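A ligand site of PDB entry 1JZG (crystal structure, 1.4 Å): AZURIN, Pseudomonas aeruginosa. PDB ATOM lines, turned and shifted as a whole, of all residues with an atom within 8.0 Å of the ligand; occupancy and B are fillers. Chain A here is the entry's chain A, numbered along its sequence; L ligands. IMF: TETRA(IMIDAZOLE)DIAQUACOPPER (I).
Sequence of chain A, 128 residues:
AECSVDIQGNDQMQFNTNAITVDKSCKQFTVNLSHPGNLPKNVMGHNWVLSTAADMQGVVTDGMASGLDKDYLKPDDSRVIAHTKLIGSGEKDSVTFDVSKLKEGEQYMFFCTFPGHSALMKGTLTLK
NZ of Lys 24 lies within salt-bridge range of OE2 of Glu 104, 3.2 Å away.
The backbone NH (N) of Val 99 lies within hydrogen-bond range of the backbone carbonyl oxygen (O) of Lys 27 (2.9 Å).
Residues that only touch the ligand: Lys 27, Val 99, Ser 100 and Leu 127.
Hydrophobic or aromatic side chains within 4 Å of the ligand: Val 99 and Leu 127.
Of the 17 residues printed, 7 come within 4 Å of the ligand.
The nearest printed residue that does not touch the ligand is Lys 103 (4.7 Å).
O1 of the ligand is in hydrogen-bond range of O of Cys 26 (2.8 Å).
O of Lys 24 sits at hydrogen-bond distance from O1 of the ligand (2.8 Å).
The backbone carbonyl oxygen (O) of Leu 102 sits at hydrogen-bond distance from a nitrogen (NDB) of the ligand (2.7 Å).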
ATOM      1  N   VAL A  22       6.036  -4.332 -11.441  1.00  0.00           N
ATOM      2  CA  VAL A  22       5.007  -5.363 -11.506  1.00  0.00           C
ATOM      3  C   VAL A  22       3.748  -4.753 -10.909  1.00  0.00           C
ATOM      4  O   VAL A  22       3.737  -4.325  -9.752  1.00  0.00           O
ATOM      5  CB  VAL A  22       5.417  -6.639 -10.726  1.00  0.00           C
ATOM      6  CG1 VAL A  22       4.254  -7.632 -10.702  1.00  0.00           C
ATOM      7  CG2 VAL A  22       6.637  -7.282 -11.375  1.00  0.00           C
ATOM      8  N   ASP A  23       2.712  -4.640 -11.728  1.00  0.00           N
ATOM      9  CA  ASP A  23       1.433  -4.067 -11.312  1.00  0.00           C
ATOM     10  C   ASP A  23       0.738  -5.038 -10.354  1.00  0.00           C
ATOM     11  O   ASP A  23       0.627  -6.230 -10.652  1.00  0.00           O
ATOM     12  CB  ASP A  23       0.555  -3.801 -12.531  1.00  0.00           C
ATOM     13  CG  ASP A  23      -0.668  -2.949 -12.225  1.00  0.00           C
ATOM     14  OD1 ASP A  23      -1.456  -3.305 -11.317  1.00  0.00           O
ATOM     15  OD2 ASP A  23      -0.860  -1.923 -12.906  1.00  0.00           O
ATOM     16  N   LYS A  24       0.250  -4.510  -9.234  1.00  0.00           N
ATOM     17  CA  LYS A  24      -0.456  -5.289  -8.215  1.00  0.00           C
ATOM     18  C   LYS A  24      -1.685  -6.019  -8.722  1.00  0.00           C
ATOM     19  O   LYS A  24      -2.192  -6.937  -8.079  1.00  0.00           O
ATOM     20  CB  LYS A  24      -0.927  -4.385  -7.080  1.00  0.00           C
ATOM     21  CG  LYS A  24       0.065  -4.139  -5.989  1.00  0.00           C
ATOM     22  CD  LYS A  24      -0.659  -3.560  -4.784  1.00  0.00           C
ATOM     23  CE  LYS A  24      -1.411  -2.269  -5.107  1.00  0.00           C
ATOM     24  NZ  LYS A  24      -1.831  -1.576  -3.866  1.00  0.00           N
ATOM     25  N   SER A  25      -2.243  -5.532  -9.831  1.00  0.00           N
ATOM     26  CA  SER A  25      -3.418  -6.144 -10.426  1.00  0.00           C
ATOM     27  C   SER A  25      -3.068  -7.500 -11.031  1.00  0.00           C
ATOM     28  O   SER A  25      -3.927  -8.371 -11.144  1.00  0.00           O
ATOM     29  CB  SER A  25      -4.029  -5.227 -11.499  1.00  0.00           C
ATOM     30  OG  SER A  25      -4.502  -4.015 -10.924  1.00  0.00           O
ATOM     31  N   CYS A  26      -1.805  -7.684 -11.396  1.00  0.00           N
ATOM     32  CA  CYS A  26      -1.346  -8.937 -11.987  1.00  0.00           C
ATOM     33  C   CYS A  26      -1.309 -10.071 -10.970  1.00  0.00           C
ATOM     34  O   CYS A  26      -0.846  -9.890  -9.849  1.00  0.00           O
ATOM     35  CB  CYS A  26       0.069  -8.777 -12.562  1.00  0.00           C
ATOM     36  SG  CYS A  26       0.254  -7.536 -13.873  1.00  0.00           S
ATOM     37  N   LYS A  27      -1.824 -11.234 -11.371  1.00  0.00           N
ATOM     38  CA  LYS A  27      -1.809 -12.434 -10.513  1.00  0.00           C
ATOM     39  C   LYS A  27      -0.515 -13.180 -10.801  1.00  0.00           C
ATOM     40  O   LYS A  27       0.059 -13.812  -9.916  1.00  0.00           O
ATOM     41  CB  LYS A  27      -3.009 -13.314 -10.797  1.00  0.00           C
ATOM     42  CG  LYS A  27      -4.250 -12.799 -10.134  1.00  0.00           C
ATOM     43  CD  LYS A  27      -5.495 -13.262 -10.825  1.00  0.00           C
ATOM     44  CE  LYS A  27      -6.677 -12.581 -10.199  1.00  0.00           C
ATOM     45  NZ  LYS A  27      -7.891 -12.611 -11.054  1.00  0.00           N
ATOM     46  N   GLN A  28      -0.115 -13.147 -12.058  1.00  0.00           N
ATOM     47  CA  GLN A  28       1.130 -13.774 -12.495  1.00  0.00           C
ATOM     48  C   GLN A  28       1.902 -12.753 -13.308  1.00  0.00           C
ATOM     49  O   GLN A  28       1.334 -11.786 -13.827  1.00  0.00           O
ATOM     50  CB  GLN A  28       0.873 -15.024 -13.351  1.00  0.00           C
ATOM     51  CG  GLN A  28       0.422 -16.250 -12.570  1.00  0.00           C
ATOM     52  CD  GLN A  28      -1.061 -16.269 -12.308  1.00  0.00           C
ATOM     53  OE1 GLN A  28      -1.846 -15.770 -13.094  1.00  0.00           O
ATOM     54  NE2 GLN A  28      -1.456 -16.848 -11.184  1.00  0.00           N
ATOM     55  N   PHE A  97       5.865 -16.347 -12.720  1.00  0.00           N
ATOM     56  CA  PHE A  97       5.784 -16.553 -11.279  1.00  0.00           C
ATOM     57  C   PHE A  97       4.567 -15.848 -10.712  1.00  0.00           C
ATOM     58  O   PHE A  97       4.007 -14.938 -11.342  1.00  0.00           O
ATOM     59  CB  PHE A  97       7.065 -16.108 -10.550  1.00  0.00           C
ATOM     60  CG  PHE A  97       7.399 -14.649 -10.721  1.00  0.00           C
ATOM     61  CD1 PHE A  97       8.164 -14.235 -11.803  1.00  0.00           C
ATOM     62  CD2 PHE A  97       6.956 -13.692  -9.808  1.00  0.00           C
ATOM     63  CE1 PHE A  97       8.468 -12.887 -11.983  1.00  0.00           C
ATOM     64  CE2 PHE A  97       7.255 -12.347  -9.980  1.00  0.00           C
ATOM     65  CZ  PHE A  97       8.013 -11.943 -11.071  1.00  0.00           C
ATOM     66  N   ASP A  98       4.138 -16.284  -9.527  1.00  0.00           N
ATOM     67  CA  ASP A  98       2.987 -15.687  -8.858  1.00  0.00           C
ATOM     68  C   ASP A  98       3.341 -14.360  -8.223  1.00  0.00           C
ATOM     69  O   ASP A  98       4.328 -14.256  -7.494  1.00  0.00           O
ATOM     70  CB  ASP A  98       2.437 -16.650  -7.810  1.00  0.00           C
ATOM     71  CG  ASP A  98       1.787 -17.864  -8.416  1.00  0.00           C
ATOM     72  OD1 ASP A  98       1.838 -18.956  -7.812  1.00  0.00           O
ATOM     73  OD2 ASP A  98       1.217 -17.736  -9.528  1.00  0.00           O
ATOM     74  N   VAL A  99       2.567 -13.327  -8.532  1.00  0.00           N
ATOM     75  CA  VAL A  99       2.804 -12.000  -7.993  1.00  0.00           C
ATOM     76  C   VAL A  99       2.683 -11.966  -6.461  1.00  0.00           C
ATOM     77  O   VAL A  99       3.303 -11.120  -5.810  1.00  0.00           O
ATOM     78  CB  VAL A  99       1.886 -10.942  -8.666  1.00  0.00           C
ATOM     79  CG1 VAL A  99       2.046  -9.591  -7.998  1.00  0.00           C
ATOM     80  CG2 VAL A  99       2.248 -10.835 -10.151  1.00  0.00           C
ATOM     81  N   SER A 100       1.984 -12.942  -5.886  1.00  0.00           N
ATOM     82  CA  SER A 100       1.852 -13.011  -4.435  1.00  0.00           C
ATOM     83  C   SER A 100       3.175 -13.410  -3.770  1.00  0.00           C
ATOM     84  O   SER A 100       3.263 -13.471  -2.549  1.00  0.00           O
ATOM     85  CB  SER A 100       0.721 -13.955  -4.015  1.00  0.00           C
ATOM     86  OG  SER A 100       0.895 -15.236  -4.538  1.00  0.00           O
ATOM     87  N   LYS A 101       4.194 -13.700  -4.584  1.00  0.00           N
ATOM     88  CA  LYS A 101       5.511 -14.012  -4.045  1.00  0.00           C
ATOM     89  C   LYS A 101       6.246 -12.700  -3.757  1.00  0.00           C
ATOM     90  O   LYS A 101       7.349 -12.707  -3.225  1.00  0.00           O
ATOM     91  CB  LYS A 101       6.318 -14.911  -5.001  1.00  0.00           C
ATOM     92  CG  LYS A 101       5.910 -16.379  -4.942  1.00  0.00           C
ATOM     93  CD  LYS A 101       6.805 -17.283  -5.772  1.00  0.00           C
ATOM     94  CE  LYS A 101       6.437 -18.753  -5.563  1.00  0.00           C
ATOM     95  NZ  LYS A 101       5.058 -19.075  -6.028  1.00  0.00           N
ATOM     96  N   LEU A 102       5.610 -11.571  -4.101  1.00  0.00           N
ATOM     97  CA  LEU A 102       6.184 -10.238  -3.873  1.00  0.00           C
ATOM     98  C   LEU A 102       5.293  -9.425  -2.933  1.00  0.00           C
ATOM     99  O   LEU A 102       4.104  -9.707  -2.798  1.00  0.00           O
ATOM    100  CB  LEU A 102       6.290  -9.473  -5.195  1.00  0.00           C
ATOM    101  CG  LEU A 102       6.945 -10.152  -6.402  1.00  0.00           C
ATOM    102  CD1 LEU A 102       6.901  -9.198  -7.584  1.00  0.00           C
ATOM    103  CD2 LEU A 102       8.366 -10.540  -6.076  1.00  0.00           C
ATOM    104  N   LYS A 103       5.878  -8.418  -2.301  1.00  0.00           N
ATOM    105  CA  LYS A 103       5.122  -7.538  -1.411  1.00  0.00           C
ATOM    106  C   LYS A 103       5.551  -6.099  -1.623  1.00  0.00           C
ATOM    107  O   LYS A 103       6.654  -5.821  -2.103  1.00  0.00           O
ATOM    108  CB  LYS A 103       5.298  -7.933   0.068  1.00  0.00           C
ATOM    109  CG  LYS A 103       6.695  -7.677   0.637  1.00  0.00           C
ATOM    110  CD  LYS A 103       6.796  -8.129   2.082  1.00  0.00           C
ATOM    111  CE  LYS A 103       8.154  -7.816   2.681  1.00  0.00           C
ATOM    112  NZ  LYS A 103       8.271  -8.281   4.079  1.00  0.00           N
ATOM    113  N   GLU A 104       4.648  -5.175  -1.306  1.00  0.00           N
ATOM    114  CA  GLU A 104       4.942  -3.751  -1.430  1.00  0.00           C
ATOM    115  C   GLU A 104       5.884  -3.353  -0.308  1.00  0.00           C
ATOM    116  O   GLU A 104       5.859  -3.942   0.781  1.00  0.00           O
ATOM    117  CB  GLU A 104       3.657  -2.939  -1.293  1.00  0.00           C
ATOM    118  CG  GLU A 104       2.662  -3.136  -2.400  1.00  0.00           C
ATOM    119  CD  GLU A 104       1.453  -2.239  -2.215  1.00  0.00           C
ATOM    120  OE1 GLU A 104       0.746  -2.408  -1.207  1.00  0.00           O
ATOM    121  OE2 GLU A 104       1.236  -1.361  -3.071  1.00  0.00           O
ATOM    122  N   TYR A 108      13.293  -5.432  -4.744  1.00  0.00           N
ATOM    123  CA  TYR A 108      13.754  -6.669  -5.377  1.00  0.00           C
ATOM    124  C   TYR A 108      14.766  -6.296  -6.445  1.00  0.00           C
ATOM    125  O   TYR A 108      14.806  -5.160  -6.909  1.00  0.00           O
ATOM    126  CB  TYR A 108      12.612  -7.430  -6.049  1.00  0.00           C
ATOM    127  CG  TYR A 108      11.531  -7.861  -5.100  1.00  0.00           C
ATOM    128  CD1 TYR A 108      11.686  -8.990  -4.301  1.00  0.00           C
ATOM    129  CD2 TYR A 108      10.405  -7.075  -4.919  1.00  0.00           C
ATOM    130  CE1 TYR A 108      10.747  -9.322  -3.334  1.00  0.00           C
ATOM    131  CE2 TYR A 108       9.451  -7.394  -3.967  1.00  0.00           C
ATOM    132  CZ  TYR A 108       9.642  -8.516  -3.168  1.00  0.00           C
ATOM    133  OH  TYR A 108       8.732  -8.798  -2.172  1.00  0.00           O
ATOM    134  N   LEU A 127       6.899  -4.035  -6.810  1.00  0.00           N
ATOM    135  CA  LEU A 127       5.466  -4.301  -6.889  1.00  0.00           C
ATOM    136  C   LEU A 127       4.770  -2.999  -6.543  1.00  0.00           C
ATOM    137  O   LEU A 127       4.999  -2.425  -5.474  1.00  0.00           O
ATOM    138  CB  LEU A 127       5.052  -5.360  -5.855  1.00  0.00           C
ATOM    139  CG  LEU A 127       3.560  -5.694  -5.838  1.00  0.00           C
ATOM    140  CD1 LEU A 127       3.200  -6.453  -7.099  1.00  0.00           C
ATOM    141  CD2 LEU A 127       3.201  -6.501  -4.600  1.00  0.00           C
HETATM  142 CU   IMF L   1      -2.452  -9.876  -4.691  1.00  0.00          CU
HETATM  143  O1  IMF L   1      -1.264  -9.425  -7.090  1.00  0.00           O
HETATM  144  CG1 IMF L   1       0.767 -10.120  -2.008  1.00  0.00           C
HETATM  145  CDC IMF L   1      -0.550 -10.211  -2.299  1.00  0.00           C
HETATM  146  NDB IMF L   1       1.386  -9.691  -3.159  1.00  0.00           N
HETATM  147  CEB IMF L   1       0.487  -9.525  -4.110  1.00  0.00           C
HETATM  148  NEC IMF L   1      -0.700  -9.829  -3.606  1.00  0.00           N
HETATM  149  CG2 IMF L   1      -2.551 -13.839  -5.945  1.00  0.00           C
HETATM  150  CDM IMF L   1      -3.075 -12.818  -5.228  1.00  0.00           C
HETATM  151  NDL IMF L   1      -1.468 -13.321  -6.624  1.00  0.00           N
HETATM  152  CEL IMF L   1      -1.338 -12.045  -6.337  1.00  0.00           C
HETATM  153  NEM IMF L   1      -2.304 -11.701  -5.491  1.00  0.00           N
